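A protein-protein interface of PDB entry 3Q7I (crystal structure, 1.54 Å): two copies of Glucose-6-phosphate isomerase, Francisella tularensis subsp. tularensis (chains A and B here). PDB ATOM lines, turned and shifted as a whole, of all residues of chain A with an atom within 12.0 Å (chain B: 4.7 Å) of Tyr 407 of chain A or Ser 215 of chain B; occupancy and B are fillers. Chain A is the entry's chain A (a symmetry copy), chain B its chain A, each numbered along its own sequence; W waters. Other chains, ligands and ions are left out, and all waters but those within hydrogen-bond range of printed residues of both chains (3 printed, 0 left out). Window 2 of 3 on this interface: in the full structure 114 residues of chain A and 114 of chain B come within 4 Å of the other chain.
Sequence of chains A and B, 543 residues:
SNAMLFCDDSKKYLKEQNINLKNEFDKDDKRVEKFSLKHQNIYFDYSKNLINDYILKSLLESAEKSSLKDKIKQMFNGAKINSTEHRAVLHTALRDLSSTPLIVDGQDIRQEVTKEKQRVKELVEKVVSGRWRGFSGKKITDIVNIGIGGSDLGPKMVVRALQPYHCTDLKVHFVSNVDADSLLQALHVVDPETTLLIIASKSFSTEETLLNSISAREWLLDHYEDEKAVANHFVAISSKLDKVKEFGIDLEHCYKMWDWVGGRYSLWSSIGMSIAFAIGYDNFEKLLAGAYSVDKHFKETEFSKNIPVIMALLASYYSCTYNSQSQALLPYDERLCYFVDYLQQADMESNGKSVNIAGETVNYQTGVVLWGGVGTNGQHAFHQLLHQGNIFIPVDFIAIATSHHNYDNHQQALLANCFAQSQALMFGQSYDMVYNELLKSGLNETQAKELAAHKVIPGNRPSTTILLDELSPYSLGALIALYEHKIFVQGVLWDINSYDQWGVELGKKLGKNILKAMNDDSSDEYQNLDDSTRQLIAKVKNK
No position is printed for both chains. Of the 10 pairs that touch across the chains among the printed residues, none has its exchanged pair printed and touching as well.
Of chain B, only Ala 180, Leu 184 and Ser 215 come within 4 Å of Tyr 407 of chain A. Of chain A, only Tyr 407 and His 410 come within 4 Å of Ser 215 of chain B. Leu 211 of chain B touches just these residues of chain A: Asn 409 (3.95 Å) and His 410 (3.6 Å). Printed residues of chain A within 4 Å of Asn 212 of chain B: His 410. No residue of chain A comes within 4 Å of Ala 216 of chain B. No residue of chain A comes within 4 Å of Glu 218 of chain B. Of the printed residues of chain B, Asn 409 of chain A touches Leu 211. Of the printed residues of chain B, His 405 of chain A touches Ala 180 (3.6 Å) and Leu 184 (3.6 Å). Printed residues of chain B within 4 Å of His 410 of chain A: Ala 180 (3.8 Å), Leu 211 (3.6 Å), Asn 212 (3.1 Å) and Ser 215 (2.7 Å). Of the printed residues of chain A, Leu 184 of chain B touches His 405 (3.6 Å) and Tyr 407 (3.9 Å). Ala 413 of chain A touches none of the printed residues of chain B. The nearest residue of chain B that does not touch Tyr 407 of chain A is Leu 187 of chain B (4.4 Å). The nearest printed residue of chain B that does not touch His 405 of chain A is Leu 183 of chain B (8.3 Å).
A ring nitrogen (NE2) of His 410 of chain A lies within hydrogen-bond range of the side-chain hydroxyl (OG) of Ser 215 of chain B (2.7 Å).
Water W3 lies within hydrogen-bond range of OE1 of Gln 411 of chain A (2.8 Å), NE2 of His 405 of chain A (2.8 Å) and N of Ala 180 of chain B (3.1 Å). Water W2 lies within hydrogen-bond range of the backbone carbonyl oxygen (O) of Ser 215 of chain B and the side-chain hydroxyl (OH) of Tyr 407 of chain A. Water W1 lies within hydrogen-bond range of the backbone carbonyl oxygen of Leu 211 of chain B (3.0 Å), the side-chain hydroxyl of Ser 215 of chain B (3.1 Å) and the side-chain amide nitrogen of Asn 409 of chain A (3.1 Å).
Hydrophobic or aromatic side chains of chain B that line the printed part of chain A: Ala 180, Leu 184 and Leu 211. Along chain B the printed residues that touch a printed residue of chain A span positions 180 to 215. Among the printed residues, no Asp or Glu carboxylate lies within 4 Å of a Lys or Arg side-chain nitrogen of the other chain.
Among the printed residues, merely in contact across the chains: His 410 of chain A with Asn 212 of chain B (3.1 Å), His 410 of chain A with Leu 211 of chain B (3.6 Å), His 405 of chain A with Leu 184 of chain B (3.6 Å), His 405 of chain A with Ala 180 of chain B (3.6 Å), Tyr 407 of chain A with Ala 180 of chain B (3.7 Å), His 410 of chain A with Ala 180 of chain B (3.8 Å), Tyr 407 of chain A with Leu 184 of chain B (3.9 Å), Tyr 407 of chain A with Ser 215 of chain B (3.9 Å) and Asn 409 of chain A with Leu 211 of chain B (3.95 Å).
The side-chain hydroxyl (OG) of Ser 403 of chain A sits close to a ring nitrogen (NE2) of His 405 of chain A. The backbone carbonyl oxygen (O) of Leu 211 of chain B sits at hydrogen-bond distance from the side-chain hydroxyl (OG) of Ser 215 of chain B, 3.2 Å away. ND1 of His 405 of chain A lies within hydrogen-bond range of N of Tyr 407 of chain A (2.9 Å).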
ATOM      1  N   TYR A 332      -3.342 -29.007 -12.404  1.00  0.00           N
ATOM      2  CA  TYR A 332      -1.895 -28.971 -12.744  1.00  0.00           C
ATOM      3  C   TYR A 332      -1.026 -28.986 -11.498  1.00  0.00           C
ATOM      4  O   TYR A 332      -0.121 -28.142 -11.281  1.00  0.00           O
ATOM      5  CB  TYR A 332      -1.603 -27.763 -13.678  1.00  0.00           C
ATOM      6  CG  TYR A 332      -1.794 -28.134 -15.144  1.00  0.00           C
ATOM      7  CD1 TYR A 332      -3.032 -28.491 -15.652  1.00  0.00           C
ATOM      8  CD2 TYR A 332      -0.694 -28.114 -16.030  1.00  0.00           C
ATOM      9  CE1 TYR A 332      -3.178 -28.837 -16.978  1.00  0.00           C
ATOM     10  CE2 TYR A 332      -0.821 -28.446 -17.354  1.00  0.00           C
ATOM     11  CZ  TYR A 332      -2.058 -28.831 -17.825  1.00  0.00           C
ATOM     12  OH  TYR A 332      -2.202 -29.184 -19.151  1.00  0.00           O
ATOM     13  N   ASP A 333      -1.256 -30.011 -10.656  1.00  0.00           N
ATOM     14  CA  ASP A 333      -0.403 -30.227  -9.467  1.00  0.00           C
ATOM     15  C   ASP A 333      -0.604 -31.641  -9.004  1.00  0.00           C
ATOM     16  O   ASP A 333      -1.747 -32.081  -8.820  1.00  0.00           O
ATOM     17  CB  ASP A 333      -0.732 -29.210  -8.363  1.00  0.00           C
ATOM     18  CG  ASP A 333       0.294 -29.172  -7.279  1.00  0.00           C
ATOM     19  OD1 ASP A 333       0.355 -30.147  -6.494  1.00  0.00           O
ATOM     20  OD2 ASP A 333       1.088 -28.193  -7.183  1.00  0.00           O
ATOM     21  N   GLU A 334       0.479 -32.334  -8.879  1.00  0.00           N
ATOM     22  CA  GLU A 334       0.516 -33.738  -8.413  1.00  0.00           C
ATOM     23  C   GLU A 334      -0.235 -33.954  -7.106  1.00  0.00           C
ATOM     24  O   GLU A 334      -0.765 -35.062  -6.888  1.00  0.00           O
ATOM     25  CB  GLU A 334       1.942 -34.136  -8.155  1.00  0.00           C
ATOM     26  CG  GLU A 334       2.755 -34.399  -9.372  1.00  0.00           C
ATOM     27  CD  GLU A 334       2.312 -35.688 -10.030  1.00  0.00           C
ATOM     28  OE1 GLU A 334       2.471 -36.791  -9.383  1.00  0.00           O
ATOM     29  OE2 GLU A 334       1.776 -35.710 -11.162  1.00  0.00           O
ATOM     30  N   ARG A 335      -0.241 -32.951  -6.222  1.00  0.00           N
ATOM     31  CA  ARG A 335      -0.858 -33.102  -4.936  1.00  0.00           C
ATOM     32  C   ARG A 335      -2.353 -33.246  -5.043  1.00  0.00           C
ATOM     33  O   ARG A 335      -2.988 -33.769  -4.120  1.00  0.00           O
ATOM     34  CB  ARG A 335      -0.469 -31.957  -4.009  1.00  0.00           C
ATOM     35  CG  ARG A 335       1.021 -31.951  -3.679  1.00  0.00           C
ATOM     36  CD  ARG A 335       1.403 -30.620  -3.012  1.00  0.00           C
ATOM     37  NE  ARG A 335       1.355 -29.504  -3.921  1.00  0.00           N
ATOM     38  CZ  ARG A 335       1.638 -28.273  -3.550  1.00  0.00           C
ATOM     39  NH1 ARG A 335       1.878 -27.949  -2.286  1.00  0.00           N
ATOM     40  NH2 ARG A 335       1.692 -27.328  -4.493  1.00  0.00           N
ATOM     41  N   ILE A 400      -1.512 -23.672  -9.754  1.00  0.00           N
ATOM     42  CA  ILE A 400      -0.970 -23.262  -8.457  1.00  0.00           C
ATOM     43  C   ILE A 400       0.289 -22.425  -8.721  1.00  0.00           C
ATOM     44  O   ILE A 400       1.254 -22.951  -9.319  1.00  0.00           O
ATOM     45  CB  ILE A 400      -0.594 -24.495  -7.590  1.00  0.00           C
ATOM     46  CG1 ILE A 400      -1.692 -25.537  -7.545  1.00  0.00           C
ATOM     47  CG2 ILE A 400      -0.157 -24.031  -6.190  1.00  0.00           C
ATOM     48  CD1 ILE A 400      -3.083 -25.101  -6.932  1.00  0.00           C
ATOM     49  N   ALA A 401       0.295 -21.144  -8.321  1.00  0.00           N
ATOM     50  CA  ALA A 401       1.380 -20.257  -8.747  1.00  0.00           C
ATOM     51  C   ALA A 401       2.741 -20.656  -8.160  1.00  0.00           C
ATOM     52  O   ALA A 401       3.766 -20.686  -8.867  1.00  0.00           O
ATOM     53  CB  ALA A 401       1.053 -18.785  -8.388  1.00  0.00           C
ATOM     54  N   THR A 402       2.736 -21.075  -6.875  1.00  0.00           N
ATOM     55  CA  THR A 402       3.974 -21.448  -6.215  1.00  0.00           C
ATOM     56  C   THR A 402       3.790 -22.762  -5.529  1.00  0.00           C
ATOM     57  O   THR A 402       2.733 -23.038  -4.970  1.00  0.00           O
ATOM     58  CB  THR A 402       4.435 -20.444  -5.224  1.00  0.00           C
ATOM     59  OG1 THR A 402       3.443 -20.324  -4.200  1.00  0.00           O
ATOM     60  CG2 THR A 402       4.715 -19.077  -5.940  1.00  0.00           C
ATOM     61  N   SER A 403       4.802 -23.621  -5.658  1.00  0.00           N
ATOM     62  CA  SER A 403       4.798 -24.969  -5.111  1.00  0.00           C
ATOM     63  C   SER A 403       5.545 -24.984  -3.797  1.00  0.00           C
ATOM     64  O   SER A 403       5.530 -23.966  -3.038  1.00  0.00           O
ATOM     65  CB  SER A 403       5.356 -25.974  -6.159  1.00  0.00           C
ATOM     66  OG  SER A 403       5.361 -27.295  -5.666  1.00  0.00           O
ATOM     67  N   HIS A 404       6.003 -26.140  -3.378  1.00  0.00           N
ATOM     68  CA  HIS A 404       6.569 -26.338  -2.056  1.00  0.00           C
ATOM     69  C   HIS A 404       8.048 -26.671  -2.074  1.00  0.00           C
ATOM     70  O   HIS A 404       8.557 -27.360  -1.185  1.00  0.00           O
ATOM     71  CB  HIS A 404       5.792 -27.435  -1.308  1.00  0.00           C
ATOM     72  CG  HIS A 404       5.869 -28.789  -1.912  1.00  0.00           C
ATOM     73  ND1 HIS A 404       6.710 -29.751  -1.407  1.00  0.00           N
ATOM     74  CD2 HIS A 404       5.224 -29.354  -2.962  1.00  0.00           C
ATOM     75  CE1 HIS A 404       6.561 -30.864  -2.126  1.00  0.00           C
ATOM     76  NE2 HIS A 404       5.671 -30.647  -3.075  1.00  0.00           N
ATOM     77  N   HIS A 405       8.730 -26.322  -3.158  1.00  0.00           N
ATOM     78  CA  HIS A 405      10.110 -26.692  -3.407  1.00  0.00           C
ATOM     79  C   HIS A 405      10.744 -25.562  -4.210  1.00  0.00           C
ATOM     80  O   HIS A 405      10.071 -24.608  -4.616  1.00  0.00           O
ATOM     81  CB  HIS A 405      10.180 -27.989  -4.192  1.00  0.00           C
ATOM     82  CG  HIS A 405       9.497 -27.894  -5.496  1.00  0.00           C
ATOM     83  ND1 HIS A 405      10.045 -27.170  -6.536  1.00  0.00           N
ATOM     84  CD2 HIS A 405       8.273 -28.283  -5.899  1.00  0.00           C
ATOM     85  CE1 HIS A 405       9.189 -27.186  -7.546  1.00  0.00           C
ATOM     86  NE2 HIS A 405       8.097 -27.849  -7.189  1.00  0.00           N
ATOM     87  N   ASN A 406      12.042 -25.691  -4.456  1.00  0.00           N
ATOM     88  CA  ASN A 406      12.835 -24.675  -5.155  1.00  0.00           C
ATOM     89  C   ASN A 406      13.313 -25.069  -6.542  1.00  0.00           C
ATOM     90  O   ASN A 406      14.270 -24.457  -7.083  1.00  0.00           O
ATOM     91  CB  ASN A 406      14.028 -24.192  -4.319  1.00  0.00           C
ATOM     92  CG  ASN A 406      13.554 -23.459  -3.080  1.00  0.00           C
ATOM     93  OD1 ASN A 406      12.775 -22.516  -3.179  1.00  0.00           O
ATOM     94  ND2 ASN A 406      13.929 -23.968  -1.915  1.00  0.00           N
ATOM     95  N   TYR A 407      12.654 -26.058  -7.130  1.00  0.00           N
ATOM     96  CA  TYR A 407      12.883 -26.400  -8.560  1.00  0.00           C
ATOM     97  C   TYR A 407      12.074 -25.459  -9.440  1.00  0.00           C
ATOM     98  O   TYR A 407      11.066 -25.791 -10.047  1.00  0.00           O
ATOM     99  CB  TYR A 407      12.544 -27.891  -8.837  1.00  0.00           C
ATOM    100  CG  TYR A 407      13.523 -28.859  -8.246  1.00  0.00           C
ATOM    101  CD1 TYR A 407      14.527 -29.382  -9.036  1.00  0.00           C
ATOM    102  CD2 TYR A 407      13.418 -29.293  -6.939  1.00  0.00           C
ATOM    103  CE1 TYR A 407      15.390 -30.307  -8.555  1.00  0.00           C
ATOM    104  CE2 TYR A 407      14.367 -30.200  -6.399  1.00  0.00           C
ATOM    105  CZ  TYR A 407      15.310 -30.716  -7.264  1.00  0.00           C
ATOM    106  OH  TYR A 407      16.224 -31.628  -6.818  1.00  0.00           O
ATOM    107  N   ASP A 408      12.533 -24.212  -9.470  1.00  0.00           N
ATOM    108  CA  ASP A 408      11.774 -23.139 -10.083  1.00  0.00           C
ATOM    109  C   ASP A 408      11.595 -23.389 -11.608  1.00  0.00           C
ATOM    110  O   ASP A 408      10.568 -23.020 -12.162  1.00  0.00           O
ATOM    111  CB  ASP A 408      12.467 -21.791  -9.830  1.00  0.00           C
ATOM    112  CG  ASP A 408      12.408 -21.334  -8.370  1.00  0.00           C
ATOM    113  OD1 ASP A 408      11.600 -21.857  -7.604  1.00  0.00           O
ATOM    114  OD2 ASP A 408      13.188 -20.373  -8.064  1.00  0.00           O
ATOM    115  N   ASN A 409      12.606 -23.979 -12.265  1.00  0.00           N
ATOM    116  CA  ASN A 409      12.454 -24.308 -13.680  1.00  0.00           C
ATOM    117  C   ASN A 409      11.325 -25.291 -13.940  1.00  0.00           C
ATOM    118  O   ASN A 409      10.584 -25.137 -14.919  1.00  0.00           O
ATOM    119  CB  ASN A 409      13.746 -24.813 -14.299  1.00  0.00           C
ATOM    120  CG  ASN A 409      14.258 -26.078 -13.690  1.00  0.00           C
ATOM    121  OD1 ASN A 409      14.115 -26.340 -12.452  1.00  0.00           O
ATOM    122  ND2 ASN A 409      14.790 -26.952 -14.589  1.00  0.00           N
ATOM    123  N   HIS A 410      11.135 -26.260 -13.031  1.00  0.00           N
ATOM    124  CA  HIS A 410      10.053 -27.209 -13.185  1.00  0.00           C
ATOM    125  C   HIS A 410       8.728 -26.495 -13.028  1.00  0.00           C
ATOM    126  O   HIS A 410       7.747 -26.753 -13.759  1.00  0.00           O
ATOM    127  CB  HIS A 410      10.194 -28.307 -12.122  1.00  0.00           C
ATOM    128  CG  HIS A 410      11.239 -29.356 -12.404  1.00  0.00           C
ATOM    129  ND1 HIS A 410      10.916 -30.661 -12.754  1.00  0.00           N
ATOM    130  CD2 HIS A 410      12.589 -29.309 -12.348  1.00  0.00           C
ATOM    131  CE1 HIS A 410      12.041 -31.356 -12.914  1.00  0.00           C
ATOM    132  NE2 HIS A 410      13.076 -30.560 -12.698  1.00  0.00           N
ATOM    133  N   GLN A 411       8.624 -25.654 -11.991  1.00  0.00           N
ATOM    134  CA  GLN A 411       7.369 -24.979 -11.683  1.00  0.00           C
ATOM    135  C   GLN A 411       6.987 -24.037 -12.854  1.00  0.00           C
ATOM    136  O   GLN A 411       5.826 -23.972 -13.241  1.00  0.00           O
ATOM    137  CB  GLN A 411       7.465 -24.252 -10.349  1.00  0.00           C
ATOM    138  CG  GLN A 411       6.184 -23.488  -9.968  1.00  0.00           C
ATOM    139  CD  GLN A 411       4.991 -24.380  -9.617  1.00  0.00           C
ATOM    140  OE1 GLN A 411       5.096 -25.614  -9.513  1.00  0.00           O
ATOM    141  NE2 GLN A 411       3.838 -23.722  -9.396  1.00  0.00           N
ATOM    142  N   GLN A 412       7.974 -23.306 -13.391  1.00  0.00           N
ATOM    143  CA  GLN A 412       7.713 -22.415 -14.506  1.00  0.00           C
ATOM    144  C   GLN A 412       7.222 -23.195 -15.730  1.00  0.00           C
ATOM    145  O   GLN A 412       6.259 -22.781 -16.371  1.00  0.00           O
ATOM    146  CB  GLN A 412       8.945 -21.607 -14.881  1.00  0.00           C
ATOM    147  CG  GLN A 412       8.564 -20.488 -15.825  1.00  0.00           C
ATOM    148  CD  GLN A 412       9.686 -19.565 -16.112  1.00  0.00           C
ATOM    149  OE1 GLN A 412      10.644 -19.991 -16.654  1.00  0.00           O
ATOM    150  NE2 GLN A 412       9.525 -18.270 -15.787  1.00  0.00           N
ATOM    151  N   ALA A 413       7.814 -24.362 -15.994  1.00  0.00           N
ATOM    152  CA  ALA A 413       7.391 -25.187 -17.094  1.00  0.00           C
ATOM    153  C   ALA A 413       5.983 -25.718 -16.908  1.00  0.00           C
ATOM    154  O   ALA A 413       5.188 -25.787 -17.860  1.00  0.00           O
ATOM    155  CB  ALA A 413       8.350 -26.353 -17.353  1.00  0.00           C
ATOM    156  N   LEU A 414       5.656 -26.126 -15.672  1.00  0.00           N
ATOM    157  CA  LEU A 414       4.326 -26.633 -15.326  1.00  0.00           C
ATOM    158  C   LEU A 414       3.267 -25.567 -15.655  1.00  0.00           C
ATOM    159  O   LEU A 414       2.298 -25.869 -16.376  1.00  0.00           O
ATOM    160  CB  LEU A 414       4.314 -27.036 -13.870  1.00  0.00           C
ATOM    161  CG  LEU A 414       2.997 -27.512 -13.292  1.00  0.00           C
ATOM    162  CD1 LEU A 414       2.459 -28.840 -13.954  1.00  0.00           C
ATOM    163  CD2 LEU A 414       3.132 -27.621 -11.711  1.00  0.00           C
ATOM    164  N   LEU A 415       3.490 -24.348 -15.205  1.00  0.00           N
ATOM    165  CA  LEU A 415       2.569 -23.229 -15.473  1.00  0.00           C
ATOM    166  C   LEU A 415       2.516 -22.844 -16.932  1.00  0.00           C
ATOM    167  O   LEU A 415       1.407 -22.636 -17.454  1.00  0.00           O
ATOM    168  CB  LEU A 415       2.916 -22.044 -14.598  1.00  0.00           C
ATOM    169  CG  LEU A 415       2.732 -22.259 -13.094  1.00  0.00           C
ATOM    170  CD1 LEU A 415       3.500 -21.179 -12.318  1.00  0.00           C
ATOM    171  CD2 LEU A 415       1.249 -22.317 -12.735  1.00  0.00           C
ATOM    172  N   ALA A 416       3.679 -22.796 -17.569  1.00  0.00           N
ATOM    173  CA  ALA A 416       3.704 -22.459 -18.994  1.00  0.00           C
ATOM    174  C   ALA A 416       2.864 -23.410 -19.794  1.00  0.00           C
ATOM    175  O   ALA A 416       2.133 -23.048 -20.712  1.00  0.00           O
ATOM    176  CB  ALA A 416       5.167 -22.429 -19.534  1.00  0.00           C
ATOM    177  N   ASN A 417       2.974 -24.692 -19.450  1.00  0.00           N
ATOM    178  CA  ASN A 417       2.185 -25.754 -20.120  1.00  0.00           C
ATOM    179  C   ASN A 417       0.688 -25.566 -19.839  1.00  0.00           C
ATOM    180  O   ASN A 417      -0.148 -25.698 -20.762  1.00  0.00           O
ATOM    181  CB  ASN A 417       2.625 -27.146 -19.693  1.00  0.00           C
ATOM    182  CG  ASN A 417       3.762 -27.664 -20.528  1.00  0.00           C
ATOM    183  OD1 ASN A 417       3.547 -28.199 -21.621  1.00  0.00           O
ATOM    184  ND2 ASN A 417       5.026 -27.426 -20.073  1.00  0.00           N
ATOM    185  N   ALA B 180       7.688 -30.774  -9.993  1.00  0.00           N
ATOM    186  CA  ALA B 180       8.787 -31.422  -9.302  1.00  0.00           C
ATOM    187  C   ALA B 180       8.351 -32.240  -8.086  1.00  0.00           C
ATOM    188  O   ALA B 180       9.103 -33.030  -7.558  1.00  0.00           O
ATOM    189  CB  ALA B 180       9.926 -30.460  -8.947  1.00  0.00           C
ATOM    190  N   LEU B 183       9.182 -35.928  -9.122  1.00  0.00           N
ATOM    191  CA  LEU B 183      10.596 -36.305  -8.883  1.00  0.00           C
ATOM    192  C   LEU B 183      10.898 -36.387  -7.406  1.00  0.00           C
ATOM    193  O   LEU B 183      11.527 -37.362  -6.961  1.00  0.00           O
ATOM    194  CB  LEU B 183      11.527 -35.256  -9.530  1.00  0.00           C
ATOM    195  CG  LEU B 183      13.048 -35.501  -9.376  1.00  0.00           C
ATOM    196  CD1 LEU B 183      13.516 -36.777 -10.003  1.00  0.00           C
ATOM    197  CD2 LEU B 183      13.819 -34.283  -9.929  1.00  0.00           C
ATOM    198  N   LEU B 184      10.397 -35.433  -6.643  1.00  0.00           N
ATOM    199  CA  LEU B 184      10.706 -35.410  -5.199  1.00  0.00           C
ATOM    200  C   LEU B 184      10.124 -36.566  -4.431  1.00  0.00           C
ATOM    201  O   LEU B 184      10.751 -37.035  -3.503  1.00  0.00           O
ATOM    202  CB  LEU B 184      10.294 -34.093  -4.570  1.00  0.00           C
ATOM    203  CG  LEU B 184      11.151 -32.921  -4.971  1.00  0.00           C
ATOM    204  CD1 LEU B 184      10.560 -31.580  -4.531  1.00  0.00           C
ATOM    205  CD2 LEU B 184      12.571 -33.003  -4.378  1.00  0.00           C
ATOM    206  N   LEU B 187      12.882 -39.075  -5.015  1.00  0.00           N
ATOM    207  CA  LEU B 187      14.192 -38.715  -4.428  1.00  0.00           C
ATOM    208  C   LEU B 187      14.145 -38.684  -2.922  1.00  0.00           C
ATOM    209  O   LEU B 187      15.139 -38.991  -2.257  1.00  0.00           O
ATOM    210  CB  LEU B 187      14.763 -37.398  -4.960  1.00  0.00           C
ATOM    211  CG  LEU B 187      14.955 -37.355  -6.475  1.00  0.00           C
ATOM    212  CD1 LEU B 187      15.613 -35.999  -6.805  1.00  0.00           C
ATOM    213  CD2 LEU B 187      15.716 -38.579  -7.031  1.00  0.00           C
ATOM    214  N   LEU B 211      13.668 -32.475 -18.423  1.00  0.00           N
ATOM    215  CA  LEU B 211      13.892 -31.695 -17.197  1.00  0.00           C
ATOM    216  C   LEU B 211      14.052 -32.655 -16.003  1.00  0.00           C
ATOM    217  O   LEU B 211      14.920 -32.445 -15.133  1.00  0.00           O
ATOM    218  CB  LEU B 211      12.782 -30.699 -16.909  1.00  0.00           C
ATOM    219  CG  LEU B 211      12.865 -29.300 -17.371  1.00  0.00           C
ATOM    220  CD1 LEU B 211      12.920 -29.219 -18.888  1.00  0.00           C
ATOM    221  CD2 LEU B 211      11.773 -28.428 -16.758  1.00  0.00           C
ATOM    222  N   ASN B 212      13.205 -33.661 -15.922  1.00  0.00           N
ATOM    223  CA  ASN B 212      13.302 -34.617 -14.828  1.00  0.00           C
ATOM    224  C   ASN B 212      14.633 -35.396 -14.834  1.00  0.00           C
ATOM    225  O   ASN B 212      15.284 -35.575 -13.806  1.00  0.00           O
ATOM    226  CB  ASN B 212      12.158 -35.615 -14.865  1.00  0.00           C
ATOM    227  CG  ASN B 212      10.843 -35.072 -14.282  1.00  0.00           C
ATOM    228  OD1 ASN B 212      10.911 -34.260 -13.361  1.00  0.00           O
ATOM    229  ND2 ASN B 212       9.703 -35.489 -14.820  1.00  0.00           N
ATOM    230  N   SER B 213      15.099 -35.792 -16.036  1.00  0.00           N
ATOM    231  CA  SER B 213      16.347 -36.546 -16.145  1.00  0.00           C
ATOM    232  C   SER B 213      17.556 -35.688 -15.810  1.00  0.00           C
ATOM    233  O   SER B 213      18.487 -36.145 -15.112  1.00  0.00           O
ATOM    234  CB  SER B 213      16.513 -37.068 -17.563  1.00  0.00           C
ATOM    235  OG  SER B 213      15.533 -38.014 -17.853  1.00  0.00           O
ATOM    236  N   ILE B 214      17.556 -34.421 -16.235  1.00  0.00           N
ATOM    237  CA  ILE B 214      18.617 -33.474 -15.894  1.00  0.00           C
ATOM    238  C   ILE B 214      18.625 -33.240 -14.390  1.00  0.00           C
ATOM    239  O   ILE B 214      19.698 -33.255 -13.759  1.00  0.00           O
ATOM    240  CB  ILE B 214      18.472 -32.168 -16.687  1.00  0.00           C
ATOM    241  CG1 ILE B 214      18.785 -32.418 -18.189  1.00  0.00           C
ATOM    242  CG2 ILE B 214      19.367 -31.078 -16.153  1.00  0.00           C
ATOM    243  CD1 ILE B 214      18.276 -31.295 -19.080  1.00  0.00           C
ATOM    244  N   SER B 215      17.442 -33.026 -13.797  1.00  0.00           N
ATOM    245  CA  SER B 215      17.402 -32.878 -12.363  1.00  0.00           C
ATOM    246  C   SER B 215      17.864 -34.109 -11.568  1.00  0.00           C
ATOM    247  O   SER B 215      18.560 -33.985 -10.567  1.00  0.00           O
ATOM    248  CB  SER B 215      16.008 -32.419 -11.930  1.00  0.00           C
ATOM    249  OG  SER B 215      15.738 -31.104 -12.397  1.00  0.00           O
ATOM    250  N   ALA B 216      17.536 -35.298 -12.057  1.00  0.00           N
ATOM    251  CA  ALA B 216      17.962 -36.524 -11.415  1.00  0.00           C
ATOM    252  C   ALA B 216      19.462 -36.690 -11.544  1.00  0.00           C
ATOM    253  O   ALA B 216      20.115 -37.132 -10.628  1.00  0.00           O
ATOM    254  CB  ALA B 216      17.228 -37.747 -12.042  1.00  0.00           C
ATOM    255  N   ARG B 217      20.021 -36.337 -12.681  1.00  0.00           N
ATOM    256  CA  ARG B 217      21.440 -36.454 -12.871  1.00  0.00           C
ATOM    257  C   ARG B 217      22.167 -35.464 -11.956  1.00  0.00           C
ATOM    258  O   ARG B 217      23.205 -35.800 -11.370  1.00  0.00           O
ATOM    259  CB  ARG B 217      21.799 -36.236 -14.347  1.00  0.00           C
ATOM    260  CG  ARG B 217      23.289 -36.388 -14.667  1.00  0.00           C
ATOM    261  CD  ARG B 217      23.517 -36.150 -16.154  1.00  0.00           C
ATOM    262  NE  ARG B 217      23.282 -34.737 -16.440  1.00  0.00           N
ATOM    263  CZ  ARG B 217      23.042 -34.200 -17.634  1.00  0.00           C
ATOM    264  NH1 ARG B 217      23.076 -34.917 -18.729  1.00  0.00           N
ATOM    265  NH2 ARG B 217      22.852 -32.897 -17.725  1.00  0.00           N
ATOM    266  N   GLU B 218      21.606 -34.262 -11.803  1.00  0.00           N
ATOM    267  CA  GLU B 218      22.194 -33.276 -10.888  1.00  0.00           C
ATOM    268  C   GLU B 218      22.183 -33.781  -9.445  1.00  0.00           C
ATOM    269  O   GLU B 218      23.149 -33.634  -8.741  1.00  0.00           O
ATOM    270  CB  GLU B 218      21.451 -31.960 -11.026  1.00  0.00           C
ATOM    271  CG  GLU B 218      21.807 -31.276 -12.282  1.00  0.00           C
ATOM    272  CD  GLU B 218      21.058 -29.956 -12.519  1.00  0.00           C
ATOM    273  OE1 GLU B 218      20.077 -29.678 -11.786  1.00  0.00           O
ATOM    274  OE2 GLU B 218      21.396 -29.252 -13.500  1.00  0.00           O
ATOM    275  N   TRP B 219      21.118 -34.461  -9.033  1.00  0.00           N
ATOM    276  CA  TRP B 219      21.028 -35.073  -7.710  1.00  0.00           C
ATOM    277  C   TRP B 219      22.088 -36.141  -7.519  1.00  0.00           C
ATOM    278  O   TRP B 219      22.779 -36.198  -6.500  1.00  0.00           O
ATOM    279  CB  TRP B 219      19.640 -35.662  -7.534  1.00  0.00           C
ATOM    280  CG  TRP B 219      19.390 -36.606  -6.453  1.00  0.00           C
ATOM    281  CD1 TRP B 219      19.082 -36.295  -5.141  1.00  0.00           C
ATOM    282  CD2 TRP B 219      19.360 -38.034  -6.540  1.00  0.00           C
ATOM    283  NE1 TRP B 219      18.850 -37.443  -4.430  1.00  0.00           N
ATOM    284  CE2 TRP B 219      18.991 -38.529  -5.252  1.00  0.00           C
ATOM    285  CE3 TRP B 219      19.516 -38.950  -7.590  1.00  0.00           C
ATOM    286  CZ2 TRP B 219      18.795 -39.894  -4.992  1.00  0.00           C
ATOM    287  CZ3 TRP B 219      19.335 -40.313  -7.313  1.00  0.00           C
ATOM    288  CH2 TRP B 219      18.951 -40.769  -6.040  1.00  0.00           C
HETATM  289  O   HOH W   1      16.126 -29.692 -15.120  1.00  0.00           O
HETATM  290  O   HOH W   2      18.425 -32.029  -8.569  1.00  0.00           O
HETATM  291  O   HOH W   3       6.443 -28.020  -9.407  1.00  0.00           O
